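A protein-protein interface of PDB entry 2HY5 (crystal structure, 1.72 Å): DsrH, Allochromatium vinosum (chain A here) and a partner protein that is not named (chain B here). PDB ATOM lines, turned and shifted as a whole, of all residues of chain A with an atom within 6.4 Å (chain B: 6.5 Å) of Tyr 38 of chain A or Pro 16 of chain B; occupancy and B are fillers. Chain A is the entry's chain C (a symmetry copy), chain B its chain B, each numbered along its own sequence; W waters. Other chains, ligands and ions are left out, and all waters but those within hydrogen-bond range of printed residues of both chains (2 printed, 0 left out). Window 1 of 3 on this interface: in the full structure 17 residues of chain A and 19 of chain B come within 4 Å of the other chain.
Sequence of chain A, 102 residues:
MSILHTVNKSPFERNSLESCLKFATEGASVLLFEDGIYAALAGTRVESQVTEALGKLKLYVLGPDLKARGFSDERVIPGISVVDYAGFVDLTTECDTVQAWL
Of the 18 printed residues of chain B, 8 touch a printed residue of chain A.
Hydrophobic or aromatic side chains of chain B within 4 Å of the printed part of chain A: Ala 15, Pro 16, Tyr 17 and Tyr 49.
Hydrophobic or aromatic side chains of chain A that line the printed part of chain B: Phe 12, Tyr 38 and Phe 71.
Among the printed residues, pairs that only touch across the chains: Tyr 38 of chain A with Tyr 49 of chain B (3.2 Å), Ala 68 of chain A with Tyr 17 of chain B (3.2 Å), Ala 68 of chain A with Gln 55 of chain B (3.3 Å), Phe 12 of chain A with Tyr 49 of chain B (3.4 Å), Tyr 38 of chain A with Ala 15 of chain B (3.4 Å), Phe 12 of chain A with Asp 46 of chain B (3.6 Å), Asp 35 of chain A with Pro 16 of chain B (3.6 Å), Tyr 38 of chain A with Pro 16 of chain B (3.6 Å), Arg 69 of chain A with Pro 16 of chain B (3.7 Å), Arg 69 of chain A with Tyr 17 of chain B (3.7 Å), Arg 69 of chain A with Gln 55 of chain B (3.8 Å), Asp 35 of chain A with Ala 15 of chain B (3.96 Å), Phe 71 of chain A with Thr 52 of chain B (3.96 Å) and Phe 71 of chain A with Tyr 49 of chain B (3.99 Å).
Water W2 lies within hydrogen-bond range of OG1 of Thr 19 of chain B, O of Ala 15 of chain B and OD1 of Asp 35 of chain A.
Water W1 lies within hydrogen-bond range of the side-chain hydroxyl (OH) of Tyr 38 of chain A (2.7 Å), the backbone carbonyl oxygen (O) of Tyr 49 of chain B (2.8 Å), the backbone carbonyl oxygen (O) of Arg 69 of chain A (2.9 Å) and the side-chain hydroxyl (OG1) of Thr 52 of chain B (3.3 Å).
The side-chain carboxylate (OD2) of Asp 35 of chain A lies close to the backbone NH (N) of Gly 18 of chain B (3.5 Å).
OG of Ser 10 of chain A lies within hydrogen-bond range of OD2 of Asp 46 of chain B (2.6 Å).
OG1 of Thr 52 of chain B lies within hydrogen-bond range of O of Arg 69 of chain A (2.8 Å).
The guanidinium group of Arg 69 of chain A lies close to the backbone NH of Gly 18 of chain B, 3.3 Å away.
OH of Tyr 17 of chain B sits at hydrogen-bond distance from OE1 of Gln 55 of chain B (2.9 Å).
OG1 of Thr 52 of chain B sits at hydrogen-bond distance from NE2 of Gln 55 of chain B, 2.9 Å away.
OG of Ser 10 of chain A sits close to N of Phe 12 of chain A, at 3.1 Å.
The side-chain carboxylate (OD2) of Asp 35 of chain A is in salt-bridge range of the guanidinium group (NH2) of Arg 69 of chain A (3.0 Å).
Of the printed residues of chain B, Phe 12 of chain A touches Asp 46 and Tyr 49.
Of chain B, only Ala 15 (3.4 Å), Pro 16 (3.6 Å) and Tyr 49 (3.2 Å) come within 4 Å of Tyr 38 of chain A.
Printed residues of chain A within 4 Å of Ala 15 of chain B: Asp 35 (3.96 Å) and Tyr 38 (3.4 Å).
Of chain A, only Asp 35 (3.6 Å), Tyr 38 (3.6 Å) and Arg 69 (3.7 Å) come within 4 Å of Pro 16 of chain B.
Of the printed residues of chain A, Tyr 17 of chain B touches Ala 68 (3.2 Å) and Arg 69 (3.7 Å).
The nearest residue of chain B that does not touch Tyr 38 of chain A is Asp 46 of chain B (5.4 Å).
The nearest printed residue of chain B that does not touch Phe 12 of chain A is Ala 15 of chain B (7.9 Å).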
ATOM      1  N   SER A  10      21.699   0.036  -8.435  1.00  0.00           N
ATOM      2  CA  SER A  10      21.730  -1.417  -8.510  1.00  0.00           C
ATOM      3  C   SER A  10      20.590  -2.028  -7.701  1.00  0.00           C
ATOM      4  O   SER A  10      20.307  -1.591  -6.584  1.00  0.00           O
ATOM      5  CB  SER A  10      23.065  -1.936  -7.972  1.00  0.00           C
ATOM      6  OG  SER A  10      23.007  -3.328  -7.728  1.00  0.00           O
ATOM      7  N   PRO A  11      19.919  -3.047  -8.259  1.00  0.00           N
ATOM      8  CA  PRO A  11      18.810  -3.713  -7.574  1.00  0.00           C
ATOM      9  C   PRO A  11      19.316  -4.580  -6.423  1.00  0.00           C
ATOM     10  O   PRO A  11      18.538  -5.032  -5.588  1.00  0.00           O
ATOM     11  CB  PRO A  11      18.168  -4.532  -8.690  1.00  0.00           C
ATOM     12  CG  PRO A  11      19.344  -4.899  -9.536  1.00  0.00           C
ATOM     13  CD  PRO A  11      20.105  -3.592  -9.616  1.00  0.00           C
ATOM     14  N   PHE A  12      20.625  -4.811  -6.388  1.00  0.00           N
ATOM     15  CA  PHE A  12      21.222  -5.622  -5.333  1.00  0.00           C
ATOM     16  C   PHE A  12      21.733  -4.709  -4.228  1.00  0.00           C
ATOM     17  O   PHE A  12      21.950  -5.137  -3.093  1.00  0.00           O
ATOM     18  CB  PHE A  12      22.382  -6.444  -5.895  1.00  0.00           C
ATOM     19  CG  PHE A  12      22.069  -7.116  -7.202  1.00  0.00           C
ATOM     20  CD1 PHE A  12      22.676  -6.693  -8.379  1.00  0.00           C
ATOM     21  CD2 PHE A  12      21.139  -8.149  -7.264  1.00  0.00           C
ATOM     22  CE1 PHE A  12      22.360  -7.285  -9.601  1.00  0.00           C
ATOM     23  CE2 PHE A  12      20.814  -8.749  -8.484  1.00  0.00           C
ATOM     24  CZ  PHE A  12      21.425  -8.315  -9.652  1.00  0.00           C
ATOM     25  N   LEU A  32      16.459   1.926 -17.191  1.00  0.00           N
ATOM     26  CA  LEU A  32      17.530   1.559 -16.285  1.00  0.00           C
ATOM     27  C   LEU A  32      18.810   2.177 -16.827  1.00  0.00           C
ATOM     28  O   LEU A  32      19.178   1.935 -17.976  1.00  0.00           O
ATOM     29  CB  LEU A  32      17.675   0.040 -16.252  1.00  0.00           C
ATOM     30  CG  LEU A  32      16.410  -0.740 -15.880  1.00  0.00           C
ATOM     31  CD1 LEU A  32      16.633  -2.237 -16.130  1.00  0.00           C
ATOM     32  CD2 LEU A  32      16.062  -0.471 -14.421  1.00  0.00           C
ATOM     33  N   GLU A  34      22.962   3.938 -15.568  1.00  0.00           N
ATOM     34  CA  GLU A  34      23.983   3.931 -14.529  1.00  0.00           C
ATOM     35  C   GLU A  34      23.999   2.522 -13.930  1.00  0.00           C
ATOM     36  O   GLU A  34      23.944   1.539 -14.666  1.00  0.00           O
ATOM     37  CB  GLU A  34      23.688   4.993 -13.461  1.00  0.00           C
ATOM     38  CG  GLU A  34      23.914   6.414 -13.963  1.00  0.00           C
ATOM     39  CD  GLU A  34      23.728   7.472 -12.891  1.00  0.00           C
ATOM     40  OE1 GLU A  34      23.839   7.138 -11.692  1.00  0.00           O
ATOM     41  OE2 GLU A  34      23.486   8.644 -13.251  1.00  0.00           O
ATOM     42  N   ASP A  35      24.060   2.419 -12.607  1.00  0.00           N
ATOM     43  CA  ASP A  35      24.094   1.115 -11.951  1.00  0.00           C
ATOM     44  C   ASP A  35      22.774   0.340 -12.035  1.00  0.00           C
ATOM     45  O   ASP A  35      22.720  -0.850 -11.703  1.00  0.00           O
ATOM     46  CB  ASP A  35      24.514   1.280 -10.486  1.00  0.00           C
ATOM     47  CG  ASP A  35      25.987   1.639 -10.334  1.00  0.00           C
ATOM     48  OD1 ASP A  35      26.405   1.937  -9.195  1.00  0.00           O
ATOM     49  OD2 ASP A  35      26.738   1.610 -11.340  1.00  0.00           O
ATOM     50  N   GLY A  36      21.709   1.008 -12.473  1.00  0.00           N
ATOM     51  CA  GLY A  36      20.430   0.331 -12.601  1.00  0.00           C
ATOM     52  C   GLY A  36      20.482  -0.732 -13.690  1.00  0.00           C
ATOM     53  O   GLY A  36      19.650  -1.646 -13.724  1.00  0.00           O
ATOM     54  N   ILE A  37      21.467  -0.602 -14.580  1.00  0.00           N
ATOM     55  CA  ILE A  37      21.687  -1.519 -15.707  1.00  0.00           C
ATOM     56  C   ILE A  37      21.776  -2.994 -15.316  1.00  0.00           C
ATOM     57  O   ILE A  37      21.344  -3.874 -16.058  1.00  0.00           O
ATOM     58  CB  ILE A  37      22.989  -1.121 -16.458  1.00  0.00           C
ATOM     59  CG1 ILE A  37      22.632  -0.456 -17.780  1.00  0.00           C
ATOM     60  CG2 ILE A  37      23.921  -2.316 -16.638  1.00  0.00           C
ATOM     61  CD1 ILE A  37      21.948   0.852 -17.613  1.00  0.00           C
ATOM     62  N   TYR A  38      22.342  -3.260 -14.148  1.00  0.00           N
ATOM     63  CA  TYR A  38      22.510  -4.635 -13.702  1.00  0.00           C
ATOM     64  C   TYR A  38      21.192  -5.403 -13.591  1.00  0.00           C
ATOM     65  O   TYR A  38      21.168  -6.624 -13.740  1.00  0.00           O
ATOM     66  CB  TYR A  38      23.257  -4.649 -12.370  1.00  0.00           C
ATOM     67  CG  TYR A  38      24.663  -4.098 -12.487  1.00  0.00           C
ATOM     68  CD1 TYR A  38      25.042  -2.944 -11.799  1.00  0.00           C
ATOM     69  CD2 TYR A  38      25.615  -4.736 -13.277  1.00  0.00           C
ATOM     70  CE1 TYR A  38      26.334  -2.443 -11.895  1.00  0.00           C
ATOM     71  CE2 TYR A  38      26.918  -4.246 -13.377  1.00  0.00           C
ATOM     72  CZ  TYR A  38      27.269  -3.095 -12.681  1.00  0.00           C
ATOM     73  OH  TYR A  38      28.554  -2.602 -12.751  1.00  0.00           O
ATOM     74  N   ALA A  39      20.103  -4.688 -13.338  1.00  0.00           N
ATOM     75  CA  ALA A  39      18.799  -5.327 -13.224  1.00  0.00           C
ATOM     76  C   ALA A  39      18.318  -5.887 -14.564  1.00  0.00           C
ATOM     77  O   ALA A  39      17.470  -6.770 -14.599  1.00  0.00           O
ATOM     78  CB  ALA A  39      17.778  -4.328 -12.683  1.00  0.00           C
ATOM     79  N   ALA A  40      18.867  -5.382 -15.663  1.00  0.00           N
ATOM     80  CA  ALA A  40      18.449  -5.837 -16.988  1.00  0.00           C
ATOM     81  C   ALA A  40      19.160  -7.099 -17.471  1.00  0.00           C
ATOM     82  O   ALA A  40      18.817  -7.651 -18.518  1.00  0.00           O
ATOM     83  CB  ALA A  40      18.651  -4.712 -17.999  1.00  0.00           C
ATOM     84  N   LEU A  41      20.137  -7.565 -16.703  1.00  0.00           N
ATOM     85  CA  LEU A  41      20.910  -8.740 -17.087  1.00  0.00           C
ATOM     86  C   LEU A  41      20.242 -10.085 -16.801  1.00  0.00           C
ATOM     87  O   LEU A  41      19.712 -10.321 -15.715  1.00  0.00           O
ATOM     88  CB  LEU A  41      22.275  -8.688 -16.406  1.00  0.00           C
ATOM     89  CG  LEU A  41      23.054  -7.400 -16.682  1.00  0.00           C
ATOM     90  CD1 LEU A  41      24.389  -7.459 -15.960  1.00  0.00           C
ATOM     91  CD2 LEU A  41      23.259  -7.223 -18.183  1.00  0.00           C
ATOM     92  N   ALA A  42      20.272 -10.970 -17.790  1.00  0.00           N
ATOM     93  CA  ALA A  42      19.678 -12.287 -17.632  1.00  0.00           C
ATOM     94  C   ALA A  42      20.487 -13.088 -16.615  1.00  0.00           C
ATOM     95  O   ALA A  42      21.699 -12.908 -16.497  1.00  0.00           O
ATOM     96  CB  ALA A  42      19.659 -13.014 -18.971  1.00  0.00           C
ATOM     97  N   THR A  44      20.302 -13.064 -13.180  1.00  0.00           N
ATOM     98  CA  THR A  44      20.484 -12.547 -11.823  1.00  0.00           C
ATOM     99  C   THR A  44      19.347 -12.982 -10.907  1.00  0.00           C
ATOM    100  O   THR A  44      18.358 -13.564 -11.356  1.00  0.00           O
ATOM    101  CB  THR A  44      20.538 -11.015 -11.784  1.00  0.00           C
ATOM    102  OG1 THR A  44      19.205 -10.495 -11.835  1.00  0.00           O
ATOM    103  CG2 THR A  44      21.348 -10.472 -12.952  1.00  0.00           C
ATOM    104  N   VAL A  46      17.218 -11.186  -9.598  1.00  0.00           N
ATOM    105  CA  VAL A  46      16.018 -10.378  -9.794  1.00  0.00           C
ATOM    106  C   VAL A  46      15.388 -10.552 -11.169  1.00  0.00           C
ATOM    107  O   VAL A  46      14.430  -9.859 -11.499  1.00  0.00           O
ATOM    108  CB  VAL A  46      16.292  -8.866  -9.569  1.00  0.00           C
ATOM    109  CG1 VAL A  46      16.861  -8.642  -8.178  1.00  0.00           C
ATOM    110  CG2 VAL A  46      17.238  -8.335 -10.633  1.00  0.00           C
ATOM    111  N   VAL A  61      16.899  -0.123 -21.269  1.00  0.00           N
ATOM    112  CA  VAL A  61      18.175  -0.093 -20.573  1.00  0.00           C
ATOM    113  C   VAL A  61      19.124   0.761 -21.402  1.00  0.00           C
ATOM    114  O   VAL A  61      19.110   0.688 -22.628  1.00  0.00           O
ATOM    115  CB  VAL A  61      18.745  -1.528 -20.393  1.00  0.00           C
ATOM    116  CG1 VAL A  61      19.002  -2.177 -21.743  1.00  0.00           C
ATOM    117  CG2 VAL A  61      20.021  -1.481 -19.575  1.00  0.00           C
ATOM    118  N   LEU A  66      25.476  -0.043 -20.069  1.00  0.00           N
ATOM    119  CA  LEU A  66      25.589  -1.496 -20.156  1.00  0.00           C
ATOM    120  C   LEU A  66      26.986  -1.869 -20.623  1.00  0.00           C
ATOM    121  O   LEU A  66      27.665  -2.690 -20.004  1.00  0.00           O
ATOM    122  CB  LEU A  66      24.582  -2.053 -21.168  1.00  0.00           C
ATOM    123  CG  LEU A  66      23.267  -2.668 -20.697  1.00  0.00           C
ATOM    124  CD1 LEU A  66      22.397  -2.940 -21.916  1.00  0.00           C
ATOM    125  CD2 LEU A  66      23.533  -3.959 -19.924  1.00  0.00           C
ATOM    126  N   ALA A  68      29.717  -0.015 -20.715  1.00  0.00           N
ATOM    127  CA  ALA A  68      30.759   0.461 -19.822  1.00  0.00           C
ATOM    128  C   ALA A  68      31.007  -0.536 -18.696  1.00  0.00           C
ATOM    129  O   ALA A  68      32.128  -0.667 -18.195  1.00  0.00           O
ATOM    130  CB  ALA A  68      30.365   1.803 -19.245  1.00  0.00           C
ATOM    131  N   ARG A  69      29.959  -1.251 -18.311  1.00  0.00           N
ATOM    132  CA  ARG A  69      30.083  -2.212 -17.231  1.00  0.00           C
ATOM    133  C   ARG A  69      30.438  -3.625 -17.680  1.00  0.00           C
ATOM    134  O   ARG A  69      30.485  -4.547 -16.868  1.00  0.00           O
ATOM    135  CB  ARG A  69      28.817  -2.169 -16.378  1.00  0.00           C
ATOM    136  CG  ARG A  69      28.740  -0.858 -15.590  1.00  0.00           C
ATOM    137  CD  ARG A  69      27.356  -0.574 -15.057  1.00  0.00           C
ATOM    138  NE  ARG A  69      27.309   0.652 -14.262  1.00  0.00           N
ATOM    139  CZ  ARG A  69      27.362   1.883 -14.765  1.00  0.00           C
ATOM    140  NH1 ARG A  69      27.470   2.071 -16.076  1.00  0.00           N
ATOM    141  NH2 ARG A  69      27.284   2.926 -13.953  1.00  0.00           N
ATOM    142  N   PHE A  71      28.908  -5.464 -20.461  1.00  0.00           N
ATOM    143  CA  PHE A  71      27.881  -6.327 -21.029  1.00  0.00           C
ATOM    144  C   PHE A  71      27.384  -5.918 -22.404  1.00  0.00           C
ATOM    145  O   PHE A  71      27.158  -4.740 -22.670  1.00  0.00           O
ATOM    146  CB  PHE A  71      26.703  -6.434 -20.060  1.00  0.00           C
ATOM    147  CG  PHE A  71      27.107  -6.859 -18.682  1.00  0.00           C
ATOM    148  CD1 PHE A  71      27.487  -5.914 -17.731  1.00  0.00           C
ATOM    149  CD2 PHE A  71      27.180  -8.208 -18.353  1.00  0.00           C
ATOM    150  CE1 PHE A  71      27.940  -6.310 -16.471  1.00  0.00           C
ATOM    151  CE2 PHE A  71      27.631  -8.613 -17.101  1.00  0.00           C
ATOM    152  CZ  PHE A  71      28.014  -7.661 -16.157  1.00  0.00           C
ATOM    153  N   LYS B  14      31.118  -1.918  -4.064  1.00  0.00           N
ATOM    154  CA  LYS B  14      30.321  -1.110  -4.981  1.00  0.00           C
ATOM    155  C   LYS B  14      30.657  -1.324  -6.453  1.00  0.00           C
ATOM    156  O   LYS B  14      31.796  -1.622  -6.816  1.00  0.00           O
ATOM    157  CB  LYS B  14      30.465   0.374  -4.628  1.00  0.00           C
ATOM    158  CG  LYS B  14      29.989   0.705  -3.221  1.00  0.00           C
ATOM    159  CD  LYS B  14      30.153   2.179  -2.912  1.00  0.00           C
ATOM    160  CE  LYS B  14      29.791   2.496  -1.467  1.00  0.00           C
ATOM    161  NZ  LYS B  14      28.375   2.171  -1.149  1.00  0.00           N
ATOM    162  N   ALA B  15      29.639  -1.198  -7.298  1.00  0.00           N
ATOM    163  CA  ALA B  15      29.817  -1.366  -8.731  1.00  0.00           C
ATOM    164  C   ALA B  15      30.607  -0.179  -9.257  1.00  0.00           C
ATOM    165  O   ALA B  15      30.542   0.914  -8.699  1.00  0.00           O
ATOM    166  CB  ALA B  15      28.453  -1.444  -9.428  1.00  0.00           C
ATOM    167  N   PRO B  16      31.369  -0.381 -10.341  1.00  0.00           N
ATOM    168  CA  PRO B  16      32.174   0.686 -10.938  1.00  0.00           C
ATOM    169  C   PRO B  16      31.344   1.689 -11.741  1.00  0.00           C
ATOM    170  O   PRO B  16      30.213   1.399 -12.143  1.00  0.00           O
ATOM    171  CB  PRO B  16      33.157  -0.089 -11.810  1.00  0.00           C
ATOM    172  CG  PRO B  16      32.318  -1.216 -12.301  1.00  0.00           C
ATOM    173  CD  PRO B  16      31.586  -1.658 -11.048  1.00  0.00           C
ATOM    174  N   TYR B  17      31.918   2.876 -11.934  1.00  0.00           N
ATOM    175  CA  TYR B  17      31.330   3.970 -12.707  1.00  0.00           C
ATOM    176  C   TYR B  17      30.153   4.747 -12.130  1.00  0.00           C
ATOM    177  O   TYR B  17      30.107   5.967 -12.264  1.00  0.00           O
ATOM    178  CB  TYR B  17      30.988   3.470 -14.112  1.00  0.00           C
ATOM    179  CG  TYR B  17      32.181   2.872 -14.805  1.00  0.00           C
ATOM    180  CD1 TYR B  17      32.243   1.504 -15.071  1.00  0.00           C
ATOM    181  CD2 TYR B  17      33.281   3.662 -15.149  1.00  0.00           C
ATOM    182  CE1 TYR B  17      33.370   0.936 -15.656  1.00  0.00           C
ATOM    183  CE2 TYR B  17      34.413   3.100 -15.735  1.00  0.00           C
ATOM    184  CZ  TYR B  17      34.451   1.739 -15.981  1.00  0.00           C
ATOM    185  OH  TYR B  17      35.581   1.177 -16.528  1.00  0.00           O
ATOM    186  N   GLY B  18      29.206   4.059 -11.502  1.00  0.00           N
ATOM    187  CA  GLY B  18      28.062   4.751 -10.916  1.00  0.00           C
ATOM    188  C   GLY B  18      28.538   5.710  -9.838  1.00  0.00           C
ATOM    189  O   GLY B  18      27.933   6.764  -9.597  1.00  0.00           O
ATOM    190  N   THR B  19      29.622   5.323  -9.176  1.00  0.00           N
ATOM    191  CA  THR B  19      30.248   6.131  -8.137  1.00  0.00           C
ATOM    192  C   THR B  19      31.754   6.018  -8.343  1.00  0.00           C
ATOM    193  O   THR B  19      32.228   5.158  -9.083  1.00  0.00           O
ATOM    194  CB  THR B  19      29.911   5.641  -6.712  1.00  0.00           C
ATOM    195  OG1 THR B  19      30.242   4.251  -6.585  1.00  0.00           O
ATOM    196  CG2 THR B  19      28.433   5.851  -6.401  1.00  0.00           C
ATOM    197  N   ALA B  22      35.019   2.697  -6.633  1.00  0.00           N
ATOM    198  CA  ALA B  22      35.825   1.630  -7.220  1.00  0.00           C
ATOM    199  C   ALA B  22      37.194   2.140  -7.661  1.00  0.00           C
ATOM    200  O   ALA B  22      38.228   1.547  -7.346  1.00  0.00           O
ATOM    201  CB  ALA B  22      35.093   1.009  -8.413  1.00  0.00           C
ATOM    202  N   TRP B  23      37.197   3.246  -8.395  1.00  0.00           N
ATOM    203  CA  TRP B  23      38.444   3.815  -8.893  1.00  0.00           C
ATOM    204  C   TRP B  23      39.336   4.385  -7.794  1.00  0.00           C
ATOM    205  O   TRP B  23      40.532   4.096  -7.748  1.00  0.00           O
ATOM    206  CB  TRP B  23      38.150   4.905  -9.930  1.00  0.00           C
ATOM    207  CG  TRP B  23      39.370   5.673 -10.340  1.00  0.00           C
ATOM    208  CD1 TRP B  23      39.536   7.027 -10.296  1.00  0.00           C
ATOM    209  CD2 TRP B  23      40.608   5.133 -10.817  1.00  0.00           C
ATOM    210  NE1 TRP B  23      40.801   7.366 -10.713  1.00  0.00           N
ATOM    211  CE2 TRP B  23      41.484   6.219 -11.041  1.00  0.00           C
ATOM    212  CE3 TRP B  23      41.068   3.834 -11.079  1.00  0.00           C
ATOM    213  CZ2 TRP B  23      42.789   6.052 -11.509  1.00  0.00           C
ATOM    214  CZ3 TRP B  23      42.370   3.666 -11.546  1.00  0.00           C
ATOM    215  CH2 TRP B  23      43.212   4.770 -11.756  1.00  0.00           C
ATOM    216  N   ASP B  46      28.139  -6.041  -4.904  1.00  0.00           N
ATOM    217  CA  ASP B  46      28.338  -5.409  -6.209  1.00  0.00           C
ATOM    218  C   ASP B  46      29.801  -5.173  -6.547  1.00  0.00           C
ATOM    219  O   ASP B  46      30.132  -4.815  -7.676  1.00  0.00           O
ATOM    220  CB  ASP B  46      27.563  -4.089  -6.319  1.00  0.00           C
ATOM    221  CG  ASP B  46      26.086  -4.299  -6.610  1.00  0.00           C
ATOM    222  OD1 ASP B  46      25.703  -5.421  -6.996  1.00  0.00           O
ATOM    223  OD2 ASP B  46      25.313  -3.328  -6.459  1.00  0.00           O
ATOM    224  N   GLY B  47      30.675  -5.376  -5.569  1.00  0.00           N
ATOM    225  CA  GLY B  47      32.093  -5.202  -5.816  1.00  0.00           C
ATOM    226  C   GLY B  47      32.603  -6.194  -6.851  1.00  0.00           C
ATOM    227  O   GLY B  47      33.594  -5.936  -7.537  1.00  0.00           O
ATOM    228  N   VAL B  48      31.933  -7.337  -6.981  1.00  0.00           N
ATOM    229  CA  VAL B  48      32.381  -8.323  -7.960  1.00  0.00           C
ATOM    230  C   VAL B  48      32.246  -7.772  -9.380  1.00  0.00           C
ATOM    231  O   VAL B  48      32.915  -8.234 -10.295  1.00  0.00           O
ATOM    232  CB  VAL B  48      31.598  -9.659  -7.847  1.00  0.00           C
ATOM    233  CG1 VAL B  48      31.708 -10.200  -6.414  1.00  0.00           C
ATOM    234  CG2 VAL B  48      30.146  -9.467  -8.243  1.00  0.00           C
ATOM    235  N   TYR B  49      31.382  -6.776  -9.556  1.00  0.00           N
ATOM    236  CA  TYR B  49      31.186  -6.167 -10.869  1.00  0.00           C
ATOM    237  C   TYR B  49      32.409  -5.348 -11.276  1.00  0.00           C
ATOM    238  O   TYR B  49      32.592  -5.021 -12.452  1.00  0.00           O
ATOM    239  CB  TYR B  49      29.943  -5.271 -10.848  1.00  0.00           C
ATOM    240  CG  TYR B  49      28.635  -6.012 -11.026  1.00  0.00           C
ATOM    241  CD1 TYR B  49      27.528  -5.707 -10.238  1.00  0.00           C
ATOM    242  CD2 TYR B  49      28.488  -6.977 -12.023  1.00  0.00           C
ATOM    243  CE1 TYR B  49      26.305  -6.336 -10.436  1.00  0.00           C
ATOM    244  CE2 TYR B  49      27.272  -7.613 -12.232  1.00  0.00           C
ATOM    245  CZ  TYR B  49      26.185  -7.286 -11.437  1.00  0.00           C
ATOM    246  OH  TYR B  49      24.977  -7.894 -11.663  1.00  0.00           O
ATOM    247  N   GLN B  50      33.245  -5.000 -10.301  1.00  0.00           N
ATOM    248  CA  GLN B  50      34.443  -4.228 -10.606  1.00  0.00           C
ATOM    249  C   GLN B  50      35.413  -5.028 -11.471  1.00  0.00           C
ATOM    250  O   GLN B  50      36.251  -4.460 -12.173  1.00  0.00           O
ATOM    251  CB  GLN B  50      35.152  -3.810  -9.316  1.00  0.00           C
ATOM    252  CG  GLN B  50      34.416  -2.772  -8.488  1.00  0.00           C
ATOM    253  CD  GLN B  50      35.233  -2.320  -7.289  1.00  0.00           C
ATOM    254  OE1 GLN B  50      36.462  -2.338  -7.326  1.00  0.00           O
ATOM    255  NE2 GLN B  50      34.557  -1.888  -6.233  1.00  0.00           N
ATOM    256  N   LEU B  51      35.293  -6.351 -11.430  1.00  0.00           N
ATOM    257  CA  LEU B  51      36.194  -7.209 -12.189  1.00  0.00           C
ATOM    258  C   LEU B  51      35.665  -7.790 -13.493  1.00  0.00           C
ATOM    259  O   LEU B  51      36.275  -8.702 -14.039  1.00  0.00           O
ATOM    260  CB  LEU B  51      36.685  -8.359 -11.305  1.00  0.00           C
ATOM    261  CG  LEU B  51      37.493  -7.986 -10.060  1.00  0.00           C
ATOM    262  CD1 LEU B  51      37.876  -9.255  -9.310  1.00  0.00           C
ATOM    263  CD2 LEU B  51      38.734  -7.208 -10.468  1.00  0.00           C
ATOM    264  N   THR B  52      34.549  -7.278 -14.003  1.00  0.00           N
ATOM    265  CA  THR B  52      34.013  -7.806 -15.253  1.00  0.00           C
ATOM    266  C   THR B  52      34.965  -7.537 -16.412  1.00  0.00           C
ATOM    267  O   THR B  52      35.660  -6.520 -16.442  1.00  0.00           O
ATOM    268  CB  THR B  52      32.632  -7.201 -15.599  1.00  0.00           C
ATOM    269  OG1 THR B  52      32.752  -5.780 -15.725  1.00  0.00           O
ATOM    270  CG2 THR B  52      31.619  -7.537 -14.521  1.00  0.00           C
ATOM    271  N   GLN B  55      34.964  -4.274 -20.478  1.00  0.00           N
ATOM    272  CA  GLN B  55      34.337  -2.985 -20.233  1.00  0.00           C
ATOM    273  C   GLN B  55      34.742  -2.016 -21.345  1.00  0.00           C
ATOM    274  O   GLN B  55      35.909  -1.961 -21.729  1.00  0.00           O
ATOM    275  CB  GLN B  55      34.771  -2.442 -18.869  1.00  0.00           C
ATOM    276  CG  GLN B  55      34.169  -3.188 -17.690  1.00  0.00           C
ATOM    277  CD  GLN B  55      34.725  -2.722 -16.357  1.00  0.00           C
ATOM    278  OE1 GLN B  55      35.376  -1.679 -16.274  1.00  0.00           O
ATOM    279  NE2 GLN B  55      34.467  -3.490 -15.305  1.00  0.00           N
ATOM    280  N   PHE B  65      39.040   2.524 -16.585  1.00  0.00           N
ATOM    281  CA  PHE B  65      40.133   2.232 -15.657  1.00  0.00           C
ATOM    282  C   PHE B  65      40.321   0.751 -15.355  1.00  0.00           C
ATOM    283  O   PHE B  65      41.211   0.379 -14.588  1.00  0.00           O
ATOM    284  CB  PHE B  65      39.962   3.004 -14.338  1.00  0.00           C
ATOM    285  CG  PHE B  65      38.758   2.597 -13.527  1.00  0.00           C
ATOM    286  CD1 PHE B  65      37.516   3.185 -13.748  1.00  0.00           C
ATOM    287  CD2 PHE B  65      38.873   1.636 -12.524  1.00  0.00           C
ATOM    288  CE1 PHE B  65      36.404   2.824 -12.973  1.00  0.00           C
ATOM    289  CE2 PHE B  65      37.771   1.270 -11.748  1.00  0.00           C
ATOM    290  CZ  PHE B  65      36.536   1.863 -11.972  1.00  0.00           C
ATOM    291  N   TYR B  69      43.223  -2.930 -12.834  1.00  0.00           N
ATOM    292  CA  TYR B  69      43.061  -4.126 -12.004  1.00  0.00           C
ATOM    293  C   TYR B  69      44.012  -5.229 -12.454  1.00  0.00           C
ATOM    294  O   TYR B  69      44.522  -5.988 -11.635  1.00  0.00           O
ATOM    295  CB  TYR B  69      41.636  -4.682 -12.076  1.00  0.00           C
ATOM    296  CG  TYR B  69      40.580  -3.813 -11.433  1.00  0.00           C
ATOM    297  CD1 TYR B  69      39.821  -2.933 -12.194  1.00  0.00           C
ATOM    298  CD2 TYR B  69      40.346  -3.868 -10.063  1.00  0.00           C
ATOM    299  CE1 TYR B  69      38.847  -2.124 -11.607  1.00  0.00           C
ATOM    300  CE2 TYR B  69      39.381  -3.065  -9.461  1.00  0.00           C
ATOM    301  CZ  TYR B  69      38.634  -2.195 -10.241  1.00  0.00           C
ATOM    302  OH  TYR B  69      37.689  -1.391  -9.651  1.00  0.00           O
HETATM  303  O   HOH W   1      30.432  -4.138 -14.019  1.00  0.00           O
HETATM  304  O   HOH W   2      28.708   2.475  -7.584  1.00  0.00           O
